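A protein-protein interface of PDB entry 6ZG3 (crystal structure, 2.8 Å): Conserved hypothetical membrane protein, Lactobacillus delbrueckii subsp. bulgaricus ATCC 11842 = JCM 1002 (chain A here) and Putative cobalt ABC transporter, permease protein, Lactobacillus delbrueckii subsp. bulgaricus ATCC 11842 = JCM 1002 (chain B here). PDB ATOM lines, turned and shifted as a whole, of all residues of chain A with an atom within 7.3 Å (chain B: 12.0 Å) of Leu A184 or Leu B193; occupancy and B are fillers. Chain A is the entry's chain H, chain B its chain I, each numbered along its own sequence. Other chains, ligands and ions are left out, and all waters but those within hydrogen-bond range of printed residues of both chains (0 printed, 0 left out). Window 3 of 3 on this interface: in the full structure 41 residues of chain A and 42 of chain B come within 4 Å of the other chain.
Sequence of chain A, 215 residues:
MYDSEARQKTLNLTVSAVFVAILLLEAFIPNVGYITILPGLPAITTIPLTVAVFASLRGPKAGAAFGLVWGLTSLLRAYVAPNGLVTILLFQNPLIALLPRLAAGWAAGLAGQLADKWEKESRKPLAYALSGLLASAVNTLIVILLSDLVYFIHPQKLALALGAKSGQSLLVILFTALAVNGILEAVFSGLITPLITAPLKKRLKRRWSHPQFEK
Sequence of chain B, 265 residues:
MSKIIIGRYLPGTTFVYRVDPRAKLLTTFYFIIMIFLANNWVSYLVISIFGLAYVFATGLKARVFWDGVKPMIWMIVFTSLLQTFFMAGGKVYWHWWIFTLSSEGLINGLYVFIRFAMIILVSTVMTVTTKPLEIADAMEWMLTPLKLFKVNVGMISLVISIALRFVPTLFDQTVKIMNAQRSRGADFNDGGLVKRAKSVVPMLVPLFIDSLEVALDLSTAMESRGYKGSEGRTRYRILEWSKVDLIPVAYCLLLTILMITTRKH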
ATOM      1  N   ILE A  35     -11.506  24.633   1.682  1.00  0.00           N
ATOM      2  CA  ILE A  35     -10.793  23.607   0.928  1.00  0.00           C
ATOM      3  C   ILE A  35      -9.295  23.866   1.068  1.00  0.00           C
ATOM      4  O   ILE A  35      -8.831  25.003   0.902  1.00  0.00           O
ATOM      5  CB  ILE A  35     -11.224  23.598  -0.548  1.00  0.00           C
ATOM      6  CG1 ILE A  35     -12.724  23.843  -0.684  1.00  0.00           C
ATOM      7  CG2 ILE A  35     -10.965  22.247  -1.143  1.00  0.00           C
ATOM      8  CD1 ILE A  35     -13.605  22.784  -0.021  1.00  0.00           C
ATOM      9  N   THR A  36      -8.536  22.818   1.378  1.00  0.00           N
ATOM     10  CA  THR A  36      -7.101  22.924   1.620  1.00  0.00           C
ATOM     11  C   THR A  36      -6.368  21.849   0.825  1.00  0.00           C
ATOM     12  O   THR A  36      -6.782  20.685   0.824  1.00  0.00           O
ATOM     13  CB  THR A  36      -6.808  22.834   3.136  1.00  0.00           C
ATOM     14  OG1 THR A  36      -5.519  23.387   3.418  1.00  0.00           O
ATOM     15  CG2 THR A  36      -6.890  21.395   3.679  1.00  0.00           C
ATOM     16  N   ILE A  37      -5.317  22.237   0.098  1.00  0.00           N
ATOM     17  CA  ILE A  37      -4.533  21.213  -0.596  1.00  0.00           C
ATOM     18  C   ILE A  37      -3.615  20.475   0.372  1.00  0.00           C
ATOM     19  O   ILE A  37      -3.493  19.242   0.320  1.00  0.00           O
ATOM     20  CB  ILE A  37      -3.714  21.839  -1.737  1.00  0.00           C
ATOM     21  CG1 ILE A  37      -4.299  23.184  -2.148  1.00  0.00           C
ATOM     22  CG2 ILE A  37      -3.638  20.881  -2.915  1.00  0.00           C
ATOM     23  CD1 ILE A  37      -5.574  23.059  -2.865  1.00  0.00           C
ATOM     24  N   ILE A  44      -8.034  28.289   1.103  1.00  0.00           N
ATOM     25  CA  ILE A  44      -9.021  29.152   0.449  1.00  0.00           C
ATOM     26  C   ILE A  44     -10.267  29.258   1.326  1.00  0.00           C
ATOM     27  O   ILE A  44     -11.005  28.287   1.519  1.00  0.00           O
ATOM     28  CB  ILE A  44      -9.380  28.663  -0.964  1.00  0.00           C
ATOM     29  CG1 ILE A  44      -9.793  27.199  -0.959  1.00  0.00           C
ATOM     30  CG2 ILE A  44      -8.231  28.887  -1.931  1.00  0.00           C
ATOM     31  CD1 ILE A  44     -11.244  27.014  -1.276  1.00  0.00           C
ATOM     32  N   SER A 136     -11.210  38.835  -2.839  1.00  0.00           N
ATOM     33  CA  SER A 136     -10.104  37.909  -2.605  1.00  0.00           C
ATOM     34  C   SER A 136      -8.754  38.500  -3.015  1.00  0.00           C
ATOM     35  O   SER A 136      -7.755  38.330  -2.303  1.00  0.00           O
ATOM     36  CB  SER A 136     -10.365  36.596  -3.351  1.00  0.00           C
ATOM     37  OG  SER A 136      -9.925  35.484  -2.589  1.00  0.00           O
ATOM     38  N   LEU A 178       0.789  32.079  -1.043  1.00  0.00           N
ATOM     39  CA  LEU A 178      -0.265  33.093  -0.976  1.00  0.00           C
ATOM     40  C   LEU A 178      -0.759  33.478  -2.359  1.00  0.00           C
ATOM     41  O   LEU A 178      -1.966  33.606  -2.574  1.00  0.00           O
ATOM     42  CB  LEU A 178       0.196  34.352  -0.229  1.00  0.00           C
ATOM     43  CG  LEU A 178       0.010  34.497   1.287  1.00  0.00           C
ATOM     44  CD1 LEU A 178       0.533  33.303   2.059  1.00  0.00           C
ATOM     45  CD2 LEU A 178       0.651  35.788   1.762  1.00  0.00           C
ATOM     46  N   ALA A 179       0.152  33.656  -3.315  1.00  0.00           N
ATOM     47  CA  ALA A 179      -0.272  34.059  -4.649  1.00  0.00           C
ATOM     48  C   ALA A 179      -1.071  32.957  -5.330  1.00  0.00           C
ATOM     49  O   ALA A 179      -2.122  33.222  -5.925  1.00  0.00           O
ATOM     50  CB  ALA A 179       0.942  34.446  -5.485  1.00  0.00           C
ATOM     51  N   VAL A 180      -0.607  31.712  -5.231  1.00  0.00           N
ATOM     52  CA  VAL A 180      -1.286  30.612  -5.917  1.00  0.00           C
ATOM     53  C   VAL A 180      -2.680  30.371  -5.320  1.00  0.00           C
ATOM     54  O   VAL A 180      -3.694  30.304  -6.045  1.00  0.00           O
ATOM     55  CB  VAL A 180      -0.402  29.349  -5.878  1.00  0.00           C
ATOM     56  CG1 VAL A 180      -1.206  28.096  -6.185  1.00  0.00           C
ATOM     57  CG2 VAL A 180       0.701  29.487  -6.881  1.00  0.00           C
ATOM     58  N   ASN A 181      -2.755  30.269  -3.985  1.00  0.00           N
ATOM     59  CA  ASN A 181      -4.044  30.159  -3.310  1.00  0.00           C
ATOM     60  C   ASN A 181      -4.926  31.355  -3.602  1.00  0.00           C
ATOM     61  O   ASN A 181      -6.144  31.207  -3.692  1.00  0.00           O
ATOM     62  CB  ASN A 181      -3.849  30.030  -1.804  1.00  0.00           C
ATOM     63  CG  ASN A 181      -3.579  28.610  -1.379  1.00  0.00           C
ATOM     64  OD1 ASN A 181      -2.425  28.185  -1.270  1.00  0.00           O
ATOM     65  ND2 ASN A 181      -4.638  27.862  -1.131  1.00  0.00           N
ATOM     66  N   GLY A 182      -4.332  32.539  -3.749  1.00  0.00           N
ATOM     67  CA  GLY A 182      -5.110  33.731  -3.984  1.00  0.00           C
ATOM     68  C   GLY A 182      -5.722  33.766  -5.356  1.00  0.00           C
ATOM     69  O   GLY A 182      -6.823  34.272  -5.518  1.00  0.00           O
ATOM     70  N   ILE A 183      -5.023  33.239  -6.358  1.00  0.00           N
ATOM     71  CA  ILE A 183      -5.617  33.146  -7.691  1.00  0.00           C
ATOM     72  C   ILE A 183      -6.758  32.142  -7.691  1.00  0.00           C
ATOM     73  O   ILE A 183      -7.848  32.417  -8.218  1.00  0.00           O
ATOM     74  CB  ILE A 183      -4.564  32.779  -8.745  1.00  0.00           C
ATOM     75  CG1 ILE A 183      -3.448  33.814  -8.754  1.00  0.00           C
ATOM     76  CG2 ILE A 183      -5.217  32.694 -10.096  1.00  0.00           C
ATOM     77  CD1 ILE A 183      -2.148  33.263  -9.242  1.00  0.00           C
ATOM     78  N   LEU A 184      -6.538  30.968  -7.082  1.00  0.00           N
ATOM     79  CA  LEU A 184      -7.639  30.016  -6.958  1.00  0.00           C
ATOM     80  C   LEU A 184      -8.834  30.646  -6.243  1.00  0.00           C
ATOM     81  O   LEU A 184      -9.944  30.700  -6.791  1.00  0.00           O
ATOM     82  CB  LEU A 184      -7.195  28.749  -6.227  1.00  0.00           C
ATOM     83  CG  LEU A 184      -6.510  27.718  -7.119  1.00  0.00           C
ATOM     84  CD1 LEU A 184      -5.209  28.230  -7.677  1.00  0.00           C
ATOM     85  CD2 LEU A 184      -6.285  26.414  -6.382  1.00  0.00           C
ATOM     86  N   GLU A 185      -8.608  31.148  -5.023  1.00  0.00           N
ATOM     87  CA  GLU A 185      -9.640  31.806  -4.222  1.00  0.00           C
ATOM     88  C   GLU A 185     -10.267  32.986  -4.950  1.00  0.00           C
ATOM     89  O   GLU A 185     -11.458  33.245  -4.791  1.00  0.00           O
ATOM     90  CB  GLU A 185      -9.034  32.268  -2.895  1.00  0.00           C
ATOM     91  CG  GLU A 185      -9.981  32.420  -1.714  1.00  0.00           C
ATOM     92  CD  GLU A 185      -9.292  33.089  -0.511  1.00  0.00           C
ATOM     93  OE1 GLU A 185      -9.224  34.344  -0.467  1.00  0.00           O
ATOM     94  OE2 GLU A 185      -8.794  32.359   0.379  1.00  0.00           O
ATOM     95  N   ALA A 186      -9.478  33.745  -5.709  1.00  0.00           N
ATOM     96  CA  ALA A 186     -10.023  34.882  -6.428  1.00  0.00           C
ATOM     97  C   ALA A 186     -11.041  34.413  -7.438  1.00  0.00           C
ATOM     98  O   ALA A 186     -12.094  35.025  -7.599  1.00  0.00           O
ATOM     99  CB  ALA A 186      -8.906  35.663  -7.114  1.00  0.00           C
ATOM    100  N   VAL A 187     -10.789  33.269  -8.065  1.00  0.00           N
ATOM    101  CA  VAL A 187     -11.739  32.823  -9.075  1.00  0.00           C
ATOM    102  C   VAL A 187     -12.947  32.139  -8.436  1.00  0.00           C
ATOM    103  O   VAL A 187     -14.092  32.372  -8.832  1.00  0.00           O
ATOM    104  CB  VAL A 187     -11.012  31.916 -10.070  1.00  0.00           C
ATOM    105  CG1 VAL A 187     -12.009  31.237 -10.995  1.00  0.00           C
ATOM    106  CG2 VAL A 187     -10.019  32.761 -10.830  1.00  0.00           C
ATOM    107  N   PHE A 188     -12.709  31.304  -7.433  1.00  0.00           N
ATOM    108  CA  PHE A 188     -13.786  30.736  -6.633  1.00  0.00           C
ATOM    109  C   PHE A 188     -14.705  31.832  -6.093  1.00  0.00           C
ATOM    110  O   PHE A 188     -15.931  31.774  -6.256  1.00  0.00           O
ATOM    111  CB  PHE A 188     -13.138  29.918  -5.526  1.00  0.00           C
ATOM    112  CG  PHE A 188     -14.056  29.440  -4.461  1.00  0.00           C
ATOM    113  CD1 PHE A 188     -14.731  28.242  -4.595  1.00  0.00           C
ATOM    114  CD2 PHE A 188     -14.163  30.133  -3.275  1.00  0.00           C
ATOM    115  CE1 PHE A 188     -15.536  27.761  -3.585  1.00  0.00           C
ATOM    116  CE2 PHE A 188     -14.966  29.664  -2.264  1.00  0.00           C
ATOM    117  CZ  PHE A 188     -15.654  28.472  -2.417  1.00  0.00           C
ATOM    118  N   SER A 189     -14.122  32.860  -5.477  1.00  0.00           N
ATOM    119  CA  SER A 189     -14.901  33.961  -4.936  1.00  0.00           C
ATOM    120  C   SER A 189     -15.523  34.817  -6.026  1.00  0.00           C
ATOM    121  O   SER A 189     -16.544  35.459  -5.778  1.00  0.00           O
ATOM    122  CB  SER A 189     -14.016  34.841  -4.038  1.00  0.00           C
ATOM    123  OG  SER A 189     -13.616  34.155  -2.855  1.00  0.00           O
ATOM    124  N   GLY A 190     -14.947  34.833  -7.230  1.00  0.00           N
ATOM    125  CA  GLY A 190     -15.519  35.626  -8.305  1.00  0.00           C
ATOM    126  C   GLY A 190     -16.650  34.918  -9.006  1.00  0.00           C
ATOM    127  O   GLY A 190     -17.491  35.563  -9.636  1.00  0.00           O
ATOM    128  N   ASP B 187     -23.130  15.450  -2.764  1.00  0.00           N
ATOM    129  CA  ASP B 187     -21.886  14.922  -2.240  1.00  0.00           C
ATOM    130  C   ASP B 187     -21.020  16.092  -1.815  1.00  0.00           C
ATOM    131  O   ASP B 187     -20.809  17.023  -2.600  1.00  0.00           O
ATOM    132  CB  ASP B 187     -21.184  14.074  -3.293  1.00  0.00           C
ATOM    133  CG  ASP B 187     -20.414  12.936  -2.688  1.00  0.00           C
ATOM    134  OD1 ASP B 187     -20.247  12.922  -1.448  1.00  0.00           O
ATOM    135  OD2 ASP B 187     -20.029  12.028  -3.453  1.00  0.00           O
ATOM    136  N   PHE B 188     -20.531  16.050  -0.570  1.00  0.00           N
ATOM    137  CA  PHE B 188     -19.724  17.134  -0.029  1.00  0.00           C
ATOM    138  C   PHE B 188     -18.261  16.782   0.198  1.00  0.00           C
ATOM    139  O   PHE B 188     -17.496  17.667   0.594  1.00  0.00           O
ATOM    140  CB  PHE B 188     -20.320  17.643   1.289  1.00  0.00           C
ATOM    141  CG  PHE B 188     -21.583  18.429   1.116  1.00  0.00           C
ATOM    142  CD1 PHE B 188     -21.594  19.574   0.331  1.00  0.00           C
ATOM    143  CD2 PHE B 188     -22.737  18.074   1.787  1.00  0.00           C
ATOM    144  CE1 PHE B 188     -22.754  20.326   0.174  1.00  0.00           C
ATOM    145  CE2 PHE B 188     -23.902  18.824   1.643  1.00  0.00           C
ATOM    146  CZ  PHE B 188     -23.908  19.954   0.835  1.00  0.00           C
ATOM    147  N   ASN B 189     -17.853  15.524  -0.018  1.00  0.00           N
ATOM    148  CA  ASN B 189     -16.432  15.145  -0.039  1.00  0.00           C
ATOM    149  C   ASN B 189     -16.263  14.029  -1.076  1.00  0.00           C
ATOM    150  O   ASN B 189     -16.308  12.845  -0.730  1.00  0.00           O
ATOM    151  CB  ASN B 189     -15.957  14.706   1.343  1.00  0.00           C
ATOM    152  CG  ASN B 189     -15.722  15.878   2.286  1.00  0.00           C
ATOM    153  OD1 ASN B 189     -16.657  16.391   2.908  1.00  0.00           O
ATOM    154  ND2 ASN B 189     -14.467  16.301   2.404  1.00  0.00           N
ATOM    155  N   ASP B 190     -16.069  14.398  -2.343  1.00  0.00           N
ATOM    156  CA  ASP B 190     -15.917  13.356  -3.354  1.00  0.00           C
ATOM    157  C   ASP B 190     -14.725  13.623  -4.270  1.00  0.00           C
ATOM    158  O   ASP B 190     -13.725  12.894  -4.236  1.00  0.00           O
ATOM    159  CB  ASP B 190     -17.207  13.195  -4.174  1.00  0.00           C
ATOM    160  CG  ASP B 190     -17.343  11.795  -4.800  1.00  0.00           C
ATOM    161  OD1 ASP B 190     -17.604  10.823  -4.051  1.00  0.00           O
ATOM    162  OD2 ASP B 190     -17.197  11.664  -6.036  1.00  0.00           O
ATOM    163  N   GLY B 191     -14.841  14.631  -5.130  1.00  0.00           N
ATOM    164  CA  GLY B 191     -13.796  14.946  -6.080  1.00  0.00           C
ATOM    165  C   GLY B 191     -12.707  15.818  -5.485  1.00  0.00           C
ATOM    166  O   GLY B 191     -12.607  16.023  -4.273  1.00  0.00           O
ATOM    167  N   GLY B 192     -11.867  16.333  -6.377  1.00  0.00           N
ATOM    168  CA  GLY B 192     -10.854  17.299  -6.014  1.00  0.00           C
ATOM    169  C   GLY B 192     -11.481  18.663  -5.833  1.00  0.00           C
ATOM    170  O   GLY B 192     -12.701  18.828  -5.880  1.00  0.00           O
ATOM    171  N   LEU B 193     -10.624  19.670  -5.638  1.00  0.00           N
ATOM    172  CA  LEU B 193     -11.133  21.031  -5.502  1.00  0.00           C
ATOM    173  C   LEU B 193     -11.979  21.432  -6.694  1.00  0.00           C
ATOM    174  O   LEU B 193     -12.865  22.285  -6.561  1.00  0.00           O
ATOM    175  CB  LEU B 193     -10.016  22.054  -5.445  1.00  0.00           C
ATOM    176  CG  LEU B 193      -8.632  21.873  -4.865  1.00  0.00           C
ATOM    177  CD1 LEU B 193      -8.025  23.243  -5.069  1.00  0.00           C
ATOM    178  CD2 LEU B 193      -8.635  21.423  -3.421  1.00  0.00           C
ATOM    179  N   VAL B 194     -11.740  20.787  -7.835  1.00  0.00           N
ATOM    180  CA  VAL B 194     -12.385  21.127  -9.098  1.00  0.00           C
ATOM    181  C   VAL B 194     -13.896  21.259  -8.927  1.00  0.00           C
ATOM    182  O   VAL B 194     -14.497  22.263  -9.321  1.00  0.00           O
ATOM    183  CB  VAL B 194     -12.006  20.078 -10.154  1.00  0.00           C
ATOM    184  CG1 VAL B 194     -10.529  20.192 -10.407  1.00  0.00           C
ATOM    185  CG2 VAL B 194     -12.296  18.666  -9.648  1.00  0.00           C
ATOM    186  N   LYS B 195     -14.537  20.207  -8.402  1.00  0.00           N
ATOM    187  CA  LYS B 195     -15.970  20.173  -8.118  1.00  0.00           C
ATOM    188  C   LYS B 195     -16.313  20.276  -6.633  1.00  0.00           C
ATOM    189  O   LYS B 195     -17.466  20.576  -6.298  1.00  0.00           O
ATOM    190  CB  LYS B 195     -16.593  18.904  -8.722  1.00  0.00           C
ATOM    191  CG  LYS B 195     -16.159  18.643 -10.188  1.00  0.00           C
ATOM    192  CD  LYS B 195     -17.336  18.287 -11.083  1.00  0.00           C
ATOM    193  CE  LYS B 195     -16.885  17.913 -12.483  1.00  0.00           C
ATOM    194  NZ  LYS B 195     -16.445  16.488 -12.602  1.00  0.00           N
ATOM    195  N   ARG B 196     -15.359  20.006  -5.738  1.00  0.00           N
ATOM    196  CA  ARG B 196     -15.578  20.323  -4.329  1.00  0.00           C
ATOM    197  C   ARG B 196     -15.881  21.798  -4.148  1.00  0.00           C
ATOM    198  O   ARG B 196     -16.585  22.173  -3.202  1.00  0.00           O
ATOM    199  CB  ARG B 196     -14.355  19.978  -3.480  1.00  0.00           C
ATOM    200  CG  ARG B 196     -14.156  18.534  -3.043  1.00  0.00           C
ATOM    201  CD  ARG B 196     -12.771  18.438  -2.378  1.00  0.00           C
ATOM    202  NE  ARG B 196     -12.740  18.910  -0.994  1.00  0.00           N
ATOM    203  CZ  ARG B 196     -11.625  19.041  -0.279  1.00  0.00           C
ATOM    204  NH1 ARG B 196     -10.446  18.734  -0.811  1.00  0.00           N
ATOM    205  NH2 ARG B 196     -11.686  19.483   0.970  1.00  0.00           N
ATOM    206  N   ALA B 197     -15.320  22.651  -5.009  1.00  0.00           N
ATOM    207  CA  ALA B 197     -15.731  24.048  -5.020  1.00  0.00           C
ATOM    208  C   ALA B 197     -17.176  24.179  -5.479  1.00  0.00           C
ATOM    209  O   ALA B 197     -17.926  25.018  -4.966  1.00  0.00           O
ATOM    210  CB  ALA B 197     -14.794  24.856  -5.920  1.00  0.00           C
ATOM    211  N   LYS B 198     -17.573  23.360  -6.460  1.00  0.00           N
ATOM    212  CA  LYS B 198     -18.930  23.419  -6.987  1.00  0.00           C
ATOM    213  C   LYS B 198     -19.956  23.135  -5.891  1.00  0.00           C
ATOM    214  O   LYS B 198     -20.979  23.822  -5.778  1.00  0.00           O
ATOM    215  CB  LYS B 198     -19.038  22.414  -8.150  1.00  0.00           C
ATOM    216  CG  LYS B 198     -18.340  22.878  -9.419  1.00  0.00           C
ATOM    217  CD  LYS B 198     -19.294  23.134 -10.550  1.00  0.00           C
ATOM    218  CE  LYS B 198     -19.489  21.856 -11.366  1.00  0.00           C
ATOM    219  NZ  LYS B 198     -20.881  21.348 -11.431  1.00  0.00           N
ATOM    220  N   SER B 199     -19.657  22.165  -5.031  1.00  0.00           N
ATOM    221  CA  SER B 199     -20.636  21.629  -4.086  1.00  0.00           C
ATOM    222  C   SER B 199     -21.060  22.614  -2.980  1.00  0.00           C
ATOM    223  O   SER B 199     -21.905  22.267  -2.141  1.00  0.00           O
ATOM    224  CB  SER B 199     -20.076  20.362  -3.442  1.00  0.00           C
ATOM    225  OG  SER B 199     -19.041  20.669  -2.523  1.00  0.00           O
ATOM    226  N   VAL B 200     -20.497  23.813  -2.919  1.00  0.00           N
ATOM    227  CA  VAL B 200     -20.828  24.701  -1.811  1.00  0.00           C
ATOM    228  C   VAL B 200     -22.120  25.481  -2.061  1.00  0.00           C
ATOM    229  O   VAL B 200     -22.771  25.909  -1.107  1.00  0.00           O
ATOM    230  CB  VAL B 200     -19.634  25.615  -1.514  1.00  0.00           C
ATOM    231  CG1 VAL B 200     -18.414  24.766  -1.226  1.00  0.00           C
ATOM    232  CG2 VAL B 200     -19.371  26.506  -2.684  1.00  0.00           C
ATOM    233  N   VAL B 201     -22.484  25.731  -3.323  1.00  0.00           N
ATOM    234  CA  VAL B 201     -23.641  26.593  -3.607  1.00  0.00           C
ATOM    235  C   VAL B 201     -24.923  26.035  -3.012  1.00  0.00           C
ATOM    236  O   VAL B 201     -25.726  26.820  -2.468  1.00  0.00           O
ATOM    237  CB  VAL B 201     -23.740  26.857  -5.116  1.00  0.00           C
ATOM    238  CG1 VAL B 201     -24.610  28.056  -5.380  1.00  0.00           C
ATOM    239  CG2 VAL B 201     -22.335  27.049  -5.729  1.00  0.00           C
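Of the 15 printed residues of chain B, 3 touch a printed residue of chain A.
Of the 18 printed residues of chain A, 4 touch a printed residue of chain B.
O of Arg B196 sits at hydrogen-bond distance from OG of Ser B199 (3.0 Å).
The backbone carbonyl oxygen of Ile A35 lies close to the backbone NH of Ile A44, at 3.4 Å.
Ile A35 touches Leu B193.
CG2 of Ile A35 touches CZ of Arg B196, 3.4 Å away.
Ile A37 touches Leu B193 (CD1 to CD1, 3.3 Å).
Leu A184 touches Leu B193 (CD2 to CD1, 3.8 Å).
Ala B197 touches Phe A188.
Leu A184 touches one residue of chain B.
Leu B193 touches just these residues of chain A: Ile A35 (3.4 Å), Ile A37 (3.3 Å) and Leu A184 (3.8 Å).
No residue of chain B comes within 4 Å of Thr A36.
Ile A37 touches one residue of chain B.
No residue of chain B comes within 4 Å of Val A180.
No residue of chain B comes within 4 Å of Gly A182.
No residue of chain B comes within 4 Å of Ile A183.
No residue of chain B comes within 4 Å of Ala A186.
No residue of chain B comes within 4 Å of Val A187.
Of the printed residues of chain A, Arg B196 touches Ile A35 (3.4 Å).
Of the printed residues of chain A, Ala B197 touches Phe A188.
Val B201 touches none of the printed residues of chain A.
Val B200 touches none of the printed residues of chain A.
The nearest residue of chain A that does not touch Leu B193 is Thr A36 (4.7 Å).
The nearest printed residue of chain A that does not touch Arg B196 is Thr A36 (4.5 Å).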
